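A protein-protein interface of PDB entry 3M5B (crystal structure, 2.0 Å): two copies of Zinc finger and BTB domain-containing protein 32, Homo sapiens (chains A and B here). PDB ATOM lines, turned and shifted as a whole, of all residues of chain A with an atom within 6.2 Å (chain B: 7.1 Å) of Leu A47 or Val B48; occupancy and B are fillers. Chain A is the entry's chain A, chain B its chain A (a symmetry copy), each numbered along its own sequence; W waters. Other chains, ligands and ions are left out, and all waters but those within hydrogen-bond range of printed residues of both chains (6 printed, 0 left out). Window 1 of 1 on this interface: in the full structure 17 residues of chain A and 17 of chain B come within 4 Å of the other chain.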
ATOM      1  N   ARG A  18      -0.139  22.193  -7.583  1.00  0.00           N
ATOM      2  CA  ARG A  18      -1.505  22.268  -7.007  1.00  0.00           C
ATOM      3  C   ARG A  18      -1.983  20.931  -6.442  1.00  0.00           C
ATOM      4  O   ARG A  18      -2.607  20.889  -5.363  1.00  0.00           O
ATOM      5  CB  ARG A  18      -2.542  22.868  -8.006  1.00  0.00           C
ATOM      6  CG  ARG A  18      -2.993  21.879  -9.061  1.00  0.00           C
ATOM      7  CD  ARG A  18      -4.338  22.206  -9.758  1.00  0.00           C
ATOM      8  NE  ARG A  18      -4.695  21.112 -10.678  1.00  0.00           N
ATOM      9  CZ  ARG A  18      -5.437  20.056 -10.334  1.00  0.00           C
ATOM     10  NH1 ARG A  18      -5.924  19.950  -9.117  1.00  0.00           N
ATOM     11  NH2 ARG A  18      -5.720  19.114 -11.214  1.00  0.00           N
ATOM     12  N   LEU A  19      -1.693  19.828  -7.141  1.00  0.00           N
ATOM     13  CA  LEU A  19      -2.094  18.511  -6.612  1.00  0.00           C
ATOM     14  C   LEU A  19      -1.261  18.098  -5.409  1.00  0.00           C
ATOM     15  O   LEU A  19      -1.761  17.404  -4.508  1.00  0.00           O
ATOM     16  CB  LEU A  19      -2.042  17.402  -7.716  1.00  0.00           C
ATOM     17  CG  LEU A  19      -3.129  16.301  -7.679  1.00  0.00           C
ATOM     18  CD1 LEU A  19      -4.594  16.816  -7.541  1.00  0.00           C
ATOM     19  CD2 LEU A  19      -3.049  15.435  -8.930  1.00  0.00           C
ATOM     20  N   ASP A  32      -2.903   5.593  -0.043  1.00  0.00           N
ATOM     21  CA  ASP A  32      -2.910   4.145  -0.387  1.00  0.00           C
ATOM     22  C   ASP A  32      -1.622   3.379   0.046  1.00  0.00           C
ATOM     23  O   ASP A  32      -1.480   2.169  -0.218  1.00  0.00           O
ATOM     24  CB  ASP A  32      -3.149   3.934  -1.906  1.00  0.00           C
ATOM     25  CG  ASP A  32      -2.084   4.581  -2.766  1.00  0.00           C
ATOM     26  OD1 ASP A  32      -1.607   5.672  -2.394  1.00  0.00           O
ATOM     27  OD2 ASP A  32      -1.733   4.028  -3.856  1.00  0.00           O
ATOM     28  N   THR A  33      -0.664   4.112   0.622  1.00  0.00           N
ATOM     29  CA  THR A  33       0.649   3.572   1.079  1.00  0.00           C
ATOM     30  C   THR A  33       0.801   3.787   2.591  1.00  0.00           C
ATOM     31  O   THR A  33       0.326   4.823   3.145  1.00  0.00           O
ATOM     32  CB  THR A  33       1.812   4.278   0.298  1.00  0.00           C
ATOM     33  OG1 THR A  33       1.617   4.088  -1.112  1.00  0.00           O
ATOM     34  CG2 THR A  33       3.196   3.735   0.693  1.00  0.00           C
ATOM     35  N   HIS A  45       0.603   9.033  -0.228  1.00  0.00           N
ATOM     36  CA  HIS A  45      -0.052   8.833  -1.550  1.00  0.00           C
ATOM     37  C   HIS A  45       1.025   8.294  -2.525  1.00  0.00           C
ATOM     38  O   HIS A  45       2.017   8.992  -2.770  1.00  0.00           O
ATOM     39  CB  HIS A  45      -0.679  10.142  -2.082  1.00  0.00           C
ATOM     40  CG  HIS A  45      -1.619  10.830  -1.120  1.00  0.00           C
ATOM     41  ND1 HIS A  45      -2.977  10.543  -1.048  1.00  0.00           N
ATOM     42  CD2 HIS A  45      -1.396  11.825  -0.211  1.00  0.00           C
ATOM     43  CE1 HIS A  45      -3.542  11.322  -0.131  1.00  0.00           C
ATOM     44  NE2 HIS A  45      -2.604  12.122   0.373  1.00  0.00           N
ATOM     45  N   SER A  46       0.871   7.040  -2.998  1.00  0.00           N
ATOM     46  CA  SER A  46       1.874   6.441  -3.895  1.00  0.00           C
ATOM     47  C   SER A  46       2.194   7.345  -5.077  1.00  0.00           C
ATOM     48  O   SER A  46       3.350   7.395  -5.513  1.00  0.00           O
ATOM     49  CB  SER A  46       1.427   5.045  -4.400  1.00  0.00           C
ATOM     50  OG  SER A  46       0.303   5.193  -5.215  1.00  0.00           O
ATOM     51  N   LEU A  47       1.175   8.044  -5.612  1.00  0.00           N
ATOM     52  CA  LEU A  47       1.324   8.952  -6.759  1.00  0.00           C
ATOM     53  C   LEU A  47       2.253  10.137  -6.475  1.00  0.00           C
ATOM     54  O   LEU A  47       3.106  10.496  -7.322  1.00  0.00           O
ATOM     55  CB  LEU A  47      -0.041   9.438  -7.337  1.00  0.00           C
ATOM     56  CG  LEU A  47      -0.037  10.485  -8.513  1.00  0.00           C
ATOM     57  CD1 LEU A  47       0.621   9.920  -9.841  1.00  0.00           C
ATOM     58  CD2 LEU A  47      -1.489  11.104  -8.812  1.00  0.00           C
ATOM     59  N   VAL A  48       2.069  10.761  -5.321  1.00  0.00           N
ATOM     60  CA  VAL A  48       3.009  11.834  -4.880  1.00  0.00           C
ATOM     61  C   VAL A  48       4.479  11.316  -4.807  1.00  0.00           C
ATOM     62  O   VAL A  48       5.418  11.953  -5.376  1.00  0.00           O
ATOM     63  CB  VAL A  48       2.504  12.524  -3.539  1.00  0.00           C
ATOM     64  CG1 VAL A  48       3.520  13.530  -2.976  1.00  0.00           C
ATOM     65  CG2 VAL A  48       1.126  13.206  -3.776  1.00  0.00           C
ATOM     66  N   LEU A  49       4.674  10.173  -4.152  1.00  0.00           N
ATOM     67  CA  LEU A  49       6.009   9.537  -4.046  1.00  0.00           C
ATOM     68  C   LEU A  49       6.677   9.242  -5.417  1.00  0.00           C
ATOM     69  O   LEU A  49       7.865   9.541  -5.642  1.00  0.00           O
ATOM     70  CB  LEU A  49       5.895   8.232  -3.234  1.00  0.00           C
ATOM     71  CG  LEU A  49       5.422   8.369  -1.755  1.00  0.00           C
ATOM     72  CD1 LEU A  49       5.366   6.996  -1.093  1.00  0.00           C
ATOM     73  CD2 LEU A  49       6.352   9.247  -1.019  1.00  0.00           C
ATOM     74  N   ALA A  50       5.883   8.702  -6.339  1.00  0.00           N
ATOM     75  CA  ALA A  50       6.339   8.405  -7.715  1.00  0.00           C
ATOM     76  C   ALA A  50       6.842   9.673  -8.441  1.00  0.00           C
ATOM     77  O   ALA A  50       7.761   9.632  -9.313  1.00  0.00           O
ATOM     78  CB  ALA A  50       5.170   7.728  -8.506  1.00  0.00           C
ATOM     79  N   GLY A  51       6.235  10.806  -8.097  1.00  0.00           N
ATOM     80  CA  GLY A  51       6.604  12.086  -8.699  1.00  0.00           C
ATOM     81  C   GLY A  51       7.980  12.603  -8.287  1.00  0.00           C
ATOM     82  O   GLY A  51       8.517  13.498  -8.928  1.00  0.00           O
ATOM     83  N   VAL A  52       8.561  12.032  -7.249  1.00  0.00           N
ATOM     84  CA  VAL A  52       9.882  12.478  -6.739  1.00  0.00           C
ATOM     85  C   VAL A  52      10.947  11.372  -6.856  1.00  0.00           C
ATOM     86  O   VAL A  52      12.139  11.645  -6.779  1.00  0.00           O
ATOM     87  CB  VAL A  52       9.758  12.881  -5.251  1.00  0.00           C
ATOM     88  CG1 VAL A  52      11.095  13.099  -4.671  1.00  0.00           C
ATOM     89  CG2 VAL A  52       8.924  14.182  -5.069  1.00  0.00           C
ATOM     90  N   GLY A  57       7.593   5.069  -5.447  1.00  0.00           N
ATOM     91  CA  GLY A  57       6.217   4.972  -6.040  1.00  0.00           C
ATOM     92  C   GLY A  57       5.631   3.558  -6.052  1.00  0.00           C
ATOM     93  O   GLY A  57       5.594   2.904  -7.074  1.00  0.00           O
ATOM     94  N   ARG B  18       2.072  18.782 -13.667  1.00  0.00           N
ATOM     95  CA  ARG B  18       3.098  17.719 -13.812  1.00  0.00           C
ATOM     96  C   ARG B  18       2.655  16.384 -13.214  1.00  0.00           C
ATOM     97  O   ARG B  18       2.897  15.315 -13.809  1.00  0.00           O
ATOM     98  CB  ARG B  18       4.491  18.156 -13.265  1.00  0.00           C
ATOM     99  CG  ARG B  18       4.582  18.098 -11.755  1.00  0.00           C
ATOM    100  CD  ARG B  18       6.016  18.027 -11.169  1.00  0.00           C
ATOM    101  NE  ARG B  18       5.943  17.873  -9.706  1.00  0.00           N
ATOM    102  CZ  ARG B  18       5.916  16.694  -9.076  1.00  0.00           C
ATOM    103  NH1 ARG B  18       5.979  15.573  -9.758  1.00  0.00           N
ATOM    104  NH2 ARG B  18       5.853  16.634  -7.760  1.00  0.00           N
ATOM    105  N   LEU B  19       1.998  16.419 -12.050  1.00  0.00           N
ATOM    106  CA  LEU B  19       1.512  15.160 -11.456  1.00  0.00           C
ATOM    107  C   LEU B  19       0.337  14.578 -12.227  1.00  0.00           C
ATOM    108  O   LEU B  19       0.174  13.349 -12.289  1.00  0.00           O
ATOM    109  CB  LEU B  19       1.138  15.335  -9.946  1.00  0.00           C
ATOM    110  CG  LEU B  19       1.440  14.156  -8.990  1.00  0.00           C
ATOM    111  CD1 LEU B  19       2.880  13.566  -9.095  1.00  0.00           C
ATOM    112  CD2 LEU B  19       1.206  14.574  -7.544  1.00  0.00           C
ATOM    113  N   VAL B  20      -0.556  15.431 -12.754  1.00  0.00           N
ATOM    114  CA  VAL B  20      -1.644  14.890 -13.604  1.00  0.00           C
ATOM    115  C   VAL B  20      -1.066  14.222 -14.863  1.00  0.00           C
ATOM    116  O   VAL B  20      -1.550  13.190 -15.280  1.00  0.00           O
ATOM    117  CB  VAL B  20      -2.682  15.975 -14.092  1.00  0.00           C
ATOM    118  CG1 VAL B  20      -3.739  15.339 -15.032  1.00  0.00           C
ATOM    119  CG2 VAL B  20      -3.369  16.646 -12.941  1.00  0.00           C
ATOM    120  N   LEU B  22       1.945  12.773 -15.211  1.00  0.00           N
ATOM    121  CA  LEU B  22       2.513  11.502 -14.754  1.00  0.00           C
ATOM    122  C   LEU B  22       1.427  10.453 -14.521  1.00  0.00           C
ATOM    123  O   LEU B  22       1.568   9.287 -14.953  1.00  0.00           O
ATOM    124  CB  LEU B  22       3.338  11.702 -13.473  1.00  0.00           C
ATOM    125  CG  LEU B  22       3.951  10.399 -12.900  1.00  0.00           C
ATOM    126  CD1 LEU B  22       4.975   9.695 -13.914  1.00  0.00           C
ATOM    127  CD2 LEU B  22       4.586  10.633 -11.485  1.00  0.00           C
ATOM    128  N   ALA B  23       0.348  10.844 -13.813  1.00  0.00           N
ATOM    129  CA  ALA B  23      -0.776   9.912 -13.584  1.00  0.00           C
ATOM    130  C   ALA B  23      -1.423   9.401 -14.918  1.00  0.00           C
ATOM    131  O   ALA B  23      -1.810   8.256 -15.041  1.00  0.00           O
ATOM    132  CB  ALA B  23      -1.850  10.588 -12.652  1.00  0.00           C
ATOM    133  N   ALA B  24      -1.533  10.277 -15.920  1.00  0.00           N
ATOM    134  CA  ALA B  24      -2.116   9.923 -17.201  1.00  0.00           C
ATOM    135  C   ALA B  24      -1.254   8.877 -17.929  1.00  0.00           C
ATOM    136  O   ALA B  24      -1.810   7.976 -18.630  1.00  0.00           O
ATOM    137  CB  ALA B  24      -2.269  11.217 -18.070  1.00  0.00           C
ATOM    138  N   LEU B  26       0.848   6.741 -16.343  1.00  0.00           N
ATOM    139  CA  LEU B  26       0.814   5.507 -15.510  1.00  0.00           C
ATOM    140  C   LEU B  26      -0.429   4.635 -15.625  1.00  0.00           C
ATOM    141  O   LEU B  26      -0.316   3.415 -15.674  1.00  0.00           O
ATOM    142  CB  LEU B  26       1.062   5.836 -14.016  1.00  0.00           C
ATOM    143  CG  LEU B  26       2.496   6.250 -13.609  1.00  0.00           C
ATOM    144  CD1 LEU B  26       2.499   6.751 -12.157  1.00  0.00           C
ATOM    145  CD2 LEU B  26       3.552   5.113 -13.839  1.00  0.00           C
ATOM    146  N   ALA B  29      -1.613   1.740 -13.666  1.00  0.00           N
ATOM    147  CA  ALA B  29      -0.665   1.549 -12.541  1.00  0.00           C
ATOM    148  C   ALA B  29      -0.907   2.572 -11.390  1.00  0.00           C
ATOM    149  O   ALA B  29      -1.116   3.755 -11.657  1.00  0.00           O
ATOM    150  CB  ALA B  29       0.780   1.621 -13.035  1.00  0.00           C
ATOM    151  N   LEU B  30      -0.926   2.070 -10.144  1.00  0.00           N
ATOM    152  CA  LEU B  30      -1.153   2.890  -8.877  1.00  0.00           C
ATOM    153  C   LEU B  30      -2.579   3.397  -8.666  1.00  0.00           C
ATOM    154  O   LEU B  30      -2.871   4.085  -7.657  1.00  0.00           O
ATOM    155  CB  LEU B  30      -0.158   4.050  -8.694  1.00  0.00           C
ATOM    156  CG  LEU B  30       1.351   3.669  -8.602  1.00  0.00           C
ATOM    157  CD1 LEU B  30       2.144   4.905  -8.440  1.00  0.00           C
ATOM    158  CD2 LEU B  30       1.694   2.608  -7.504  1.00  0.00           C
ATOM    159  N   ASP B  32      -6.131   3.529  -7.335  1.00  0.00           N
ATOM    160  CA  ASP B  32      -6.809   2.989  -6.124  1.00  0.00           C
ATOM    161  C   ASP B  32      -8.366   2.973  -6.217  1.00  0.00           C
ATOM    162  O   ASP B  32      -9.058   2.584  -5.256  1.00  0.00           O
ATOM    163  CB  ASP B  32      -6.375   3.763  -4.850  1.00  0.00           C
ATOM    164  CG  ASP B  32      -6.710   5.238  -4.915  1.00  0.00           C
ATOM    165  OD1 ASP B  32      -6.611   5.818  -6.015  1.00  0.00           O
ATOM    166  OD2 ASP B  32      -7.038   5.856  -3.853  1.00  0.00           O
ATOM    167  N   ALA B  44      -8.905   4.509 -11.936  1.00  0.00           N
ATOM    168  CA  ALA B  44      -8.535   5.936 -11.745  1.00  0.00           C
ATOM    169  C   ALA B  44      -7.802   6.151 -10.422  1.00  0.00           C
ATOM    170  O   ALA B  44      -7.856   5.302  -9.522  1.00  0.00           O
ATOM    171  CB  ALA B  44      -9.797   6.861 -11.817  1.00  0.00           C
ATOM    172  N   HIS B  45      -7.149   7.317 -10.297  1.00  0.00           N
ATOM    173  CA  HIS B  45      -6.414   7.747  -9.075  1.00  0.00           C
ATOM    174  C   HIS B  45      -7.356   8.677  -8.271  1.00  0.00           C
ATOM    175  O   HIS B  45      -7.745   9.732  -8.789  1.00  0.00           O
ATOM    176  CB  HIS B  45      -5.090   8.463  -9.425  1.00  0.00           C
ATOM    177  CG  HIS B  45      -4.179   7.691 -10.351  1.00  0.00           C
ATOM    178  ND1 HIS B  45      -3.235   6.777  -9.899  1.00  0.00           N
ATOM    179  CD2 HIS B  45      -4.047   7.729 -11.710  1.00  0.00           C
ATOM    180  CE1 HIS B  45      -2.572   6.280 -10.940  1.00  0.00           C
ATOM    181  NE2 HIS B  45      -3.035   6.862 -12.045  1.00  0.00           N
ATOM    182  N   SER B  46      -7.782   8.248  -7.065  1.00  0.00           N
ATOM    183  CA  SER B  46      -8.713   9.057  -6.259  1.00  0.00           C
ATOM    184  C   SER B  46      -8.228  10.490  -6.095  1.00  0.00           C
ATOM    185  O   SER B  46      -9.048  11.415  -6.083  1.00  0.00           O
ATOM    186  CB  SER B  46      -8.966   8.419  -4.868  1.00  0.00           C
ATOM    187  OG  SER B  46      -7.781   8.448  -4.130  1.00  0.00           O
ATOM    188  N   LEU B  47      -6.903  10.679  -5.947  1.00  0.00           N
ATOM    189  CA  LEU B  47      -6.284  12.002  -5.771  1.00  0.00           C
ATOM    190  C   LEU B  47      -6.487  12.928  -6.975  1.00  0.00           C
ATOM    191  O   LEU B  47      -6.801  14.131  -6.808  1.00  0.00           O
ATOM    192  CB  LEU B  47      -4.778  11.926  -5.371  1.00  0.00           C
ATOM    193  CG  LEU B  47      -3.961  13.264  -5.234  1.00  0.00           C
ATOM    194  CD1 LEU B  47      -4.492  14.196  -4.066  1.00  0.00           C
ATOM    195  CD2 LEU B  47      -2.378  13.026  -5.102  1.00  0.00           C
ATOM    196  N   VAL B  48      -6.272  12.393  -8.168  1.00  0.00           N
ATOM    197  CA  VAL B  48      -6.577  13.161  -9.411  1.00  0.00           C
ATOM    198  C   VAL B  48      -8.071  13.613  -9.454  1.00  0.00           C
ATOM    199  O   VAL B  48      -8.374  14.823  -9.690  1.00  0.00           O
ATOM    200  CB  VAL B  48      -6.109  12.367 -10.706  1.00  0.00           C
ATOM    201  CG1 VAL B  48      -6.540  13.059 -12.008  1.00  0.00           C
ATOM    202  CG2 VAL B  48      -4.567  12.161 -10.676  1.00  0.00           C
ATOM    203  N   LEU B  49      -8.982  12.675  -9.203  1.00  0.00           N
ATOM    204  CA  LEU B  49     -10.434  12.971  -9.161  1.00  0.00           C
ATOM    205  C   LEU B  49     -10.822  14.079  -8.144  1.00  0.00           C
ATOM    206  O   LEU B  49     -11.586  15.012  -8.456  1.00  0.00           O
ATOM    207  CB  LEU B  49     -11.214  11.680  -8.843  1.00  0.00           C
ATOM    208  CG  LEU B  49     -11.094  10.519  -9.875  1.00  0.00           C
ATOM    209  CD1 LEU B  49     -11.922   9.322  -9.418  1.00  0.00           C
ATOM    210  CD2 LEU B  49     -11.562  10.982 -11.196  1.00  0.00           C
ATOM    211  N   ALA B  50     -10.245  13.989  -6.948  1.00  0.00           N
ATOM    212  CA  ALA B  50     -10.460  14.989  -5.878  1.00  0.00           C
ATOM    213  C   ALA B  50     -10.037  16.407  -6.322  1.00  0.00           C
ATOM    214  O   ALA B  50     -10.611  17.450  -5.887  1.00  0.00           O
ATOM    215  CB  ALA B  50      -9.678  14.542  -4.597  1.00  0.00           C
ATOM    216  N   GLY B  51      -9.022  16.458  -7.182  1.00  0.00           N
ATOM    217  CA  GLY B  51      -8.513  17.729  -7.691  1.00  0.00           C
ATOM    218  C   GLY B  51      -9.463  18.454  -8.643  1.00  0.00           C
ATOM    219  O   GLY B  51      -9.284  19.636  -8.906  1.00  0.00           O
ATOM    220  N   VAL B  52     -10.476  17.766  -9.133  1.00  0.00           N
ATOM    221  CA  VAL B  52     -11.440  18.358 -10.095  1.00  0.00           C
ATOM    222  C   VAL B  52     -12.868  18.411  -9.520  1.00  0.00           C
ATOM    223  O   VAL B  52     -13.717  19.132 -10.029  1.00  0.00           O
ATOM    224  CB  VAL B  52     -11.467  17.514 -11.392  1.00  0.00           C
ATOM    225  CG1 VAL B  52     -12.581  17.947 -12.254  1.00  0.00           C
ATOM    226  CG2 VAL B  52     -10.142  17.643 -12.195  1.00  0.00           C
ATOM    227  N   SER B  53     -13.177  17.542  -8.556  1.00  0.00           N
ATOM    228  CA  SER B  53     -14.536  17.429  -8.016  1.00  0.00           C
ATOM    229  C   SER B  53     -14.504  16.737  -6.671  1.00  0.00           C
ATOM    230  O   SER B  53     -14.122  15.558  -6.605  1.00  0.00           O
ATOM    231  CB  SER B  53     -15.380  16.570  -8.962  1.00  0.00           C
ATOM    232  OG  SER B  53     -16.592  16.128  -8.381  1.00  0.00           O
ATOM    233  N   GLY B  57     -13.762  12.375  -5.554  1.00  0.00           N
ATOM    234  CA  GLY B  57     -12.550  11.994  -4.754  1.00  0.00           C
ATOM    235  C   GLY B  57     -12.812  10.946  -3.669  1.00  0.00           C
ATOM    236  O   GLY B  57     -12.891  11.261  -2.500  1.00  0.00           O
ATOM    237  N   LEU B  77     -13.507  11.269 -18.298  1.00  0.00           N
ATOM    238  CA  LEU B  77     -12.273  10.812 -17.630  1.00  0.00           C
ATOM    239  C   LEU B  77     -11.005  11.234 -18.386  1.00  0.00           C
ATOM    240  O   LEU B  77     -10.068  11.730 -17.775  1.00  0.00           O
ATOM    241  CB  LEU B  77     -12.307   9.289 -17.359  1.00  0.00           C
ATOM    242  CG  LEU B  77     -11.286   8.696 -16.374  1.00  0.00           C
ATOM    243  CD1 LEU B  77     -11.366   9.406 -14.999  1.00  0.00           C
ATOM    244  CD2 LEU B  77     -11.473   7.175 -16.201  1.00  0.00           C
ATOM    245  N   VAL B  80     -10.404  14.967 -17.619  1.00  0.00           N
ATOM    246  CA  VAL B  80      -9.867  15.086 -16.245  1.00  0.00           C
ATOM    247  C   VAL B  80      -8.352  14.781 -16.166  1.00  0.00           C
ATOM    248  O   VAL B  80      -7.639  15.398 -15.356  1.00  0.00           O
ATOM    249  CB  VAL B  80     -10.722  14.205 -15.262  1.00  0.00           C
ATOM    250  CG1 VAL B  80     -10.042  14.042 -13.866  1.00  0.00           C
ATOM    251  CG2 VAL B  80     -12.176  14.793 -15.142  1.00  0.00           C
ATOM    252  N   TYR B  81      -7.880  13.862 -17.007  1.00  0.00           N
ATOM    253  CA  TYR B  81      -6.453  13.464 -17.102  1.00  0.00           C
ATOM    254  C   TYR B  81      -5.616  14.332 -18.100  1.00  0.00           C
ATOM    255  O   TYR B  81      -4.422  14.028 -18.361  1.00  0.00           O
ATOM    256  CB  TYR B  81      -6.349  11.966 -17.475  1.00  0.00           C
ATOM    257  CG  TYR B  81      -6.379  11.023 -16.265  1.00  0.00           C
ATOM    258  CD1 TYR B  81      -5.221  10.807 -15.483  1.00  0.00           C
ATOM    259  CD2 TYR B  81      -7.547  10.356 -15.908  1.00  0.00           C
ATOM    260  CE1 TYR B  81      -5.237   9.930 -14.370  1.00  0.00           C
ATOM    261  CE2 TYR B  81      -7.590   9.448 -14.786  1.00  0.00           C
ATOM    262  CZ  TYR B  81      -6.417   9.253 -14.033  1.00  0.00           C
ATOM    263  OH  TYR B  81      -6.438   8.427 -12.940  1.00  0.00           O
ATOM    264  N   GLY B  82      -6.225  15.397 -18.643  1.00  0.00           N
ATOM    265  CA  GLY B  82      -5.477  16.409 -19.394  1.00  0.00           C
ATOM    266  C   GLY B  82      -5.552  16.251 -20.912  1.00  0.00           C
ATOM    267  O   GLY B  82      -4.855  16.955 -21.637  1.00  0.00           O
HETATM  268  O   HOH W   1      -6.953  16.973 -13.299  1.00  0.00           O
HETATM  269  O   HOH W   2      -3.101   2.403  -5.277  1.00  0.00           O
HETATM  270  O   HOH W   3      -6.613  16.924 -10.540  1.00  0.00           O
HETATM  271  O   HOH W   4       5.277  14.557  -6.575  1.00  0.00           O
HETATM  272  O   HOH W   5      -7.177  21.417  -7.591  1.00  0.00           O
HETATM  273  O   HOH W   6       7.428  14.672 -11.531  1.00  0.00           O
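The side-chain carboxylate (OD2) of Asp A32 sits at hydrogen-bond distance from the side-chain hydroxyl (OG) of Ser A46 (2.7 Å).
Of the printed residues of chain B, Leu A19 touches Leu B47. Leu A47 touches three residues of chain B. Printed residues of chain A within 4 Å of Val B20: Arg A18. Printed residues of chain A within 4 Å of Leu B47: Leu A19 (3.6 Å) and Val A48 (3.8 Å). Printed residues of chain A within 4 Å of Val B48: Leu A47 (3.8 Å). Printed residues of chain A within 4 Å of Gly B51: Arg A18 (3.4 Å). The nearest printed residue of chain A that does not touch Val B48 is Leu A19 (4.01 Å).
Arg A18 touches Gly B51, and with the chains exchanged Gly A51 touches Arg B18. Leu A19 touches Leu B47, and with the chains exchanged Leu A47 touches Leu B19. Leu A47 touches Val B48, and with the chains exchanged Val A48 touches Leu B47. Of the 13 pairs that touch across the chains among the printed residues, 6 have their exchanged pair printed and touching as well.
Water W4 bridges the guanidinium group (NH2) of Arg B18 and the backbone carbonyl oxygen (O) of Val A48. Water W3 bridges NH2 of Arg A18 (2.5 Å) and O of Val B48 (2.9 Å). Water W5 bridges the guanidinium group of Arg A18 (2.5 Å) and the backbone carbonyl oxygen of Gly B51 (3.1 Å). Water W6 bridges NH1 of Arg B18 (2.5 Å) and O of Gly A51 (3.1 Å). Water W2 bridges OD2 of Asp A32 (2.6 Å) and O of Leu B30 (2.9 Å). Water W1 lies within hydrogen-bond range of O of Val B80 (2.7 Å) and NH2 of Arg A18 (3.2 Å).
Printed residues of chain A that touch a printed residue of chain B: Arg A18, Leu A19, Asp A32, Ser A46, Leu A47, Val A48, Ala A50, Gly A51 and Gly A57. Hydrophobic or aromatic side chains of chain A that line the printed part of chain B: Leu A19, Leu A47 and Val A48. Hydrophobic or aromatic side chains of chain B within 4 Å of the printed part of chain A: Leu B19, Val B20, Leu B22, Ala B23, Leu B30, Leu B47 and Val B48. Among the printed residues, no Asp or Glu carboxylate lies within 4 Å of a Lys or Arg side-chain nitrogen of the other chain.
The backbone carbonyl oxygen of Gly B51 sits at hydrogen-bond distance from the guanidinium group of Arg A18. The backbone carbonyl oxygen of Gly A51 lies within hydrogen-bond range of the guanidinium group of Arg B18 (3.4 Å).
Among the printed residues, pairs that only touch across the chains: Leu A19 with Leu B47 (3.6 Å), Leu A47 with Leu B19 (3.6 Å), Ser A46 with Leu B30 (3.7 Å), Gly A51 with Leu B22 (3.7 Å), Leu A47 with Val B48 (3.8 Å), Val A48 with Leu B47 (3.8 Å), Leu A47 with Ala B23 (3.8 Å), Arg A18 with Val B20 (3.8 Å), Ala A50 with Leu B22 (3.9 Å), Gly A57 with Leu B30 (3.9 Å) and Asp A32 with Leu B30 (3.97 Å).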
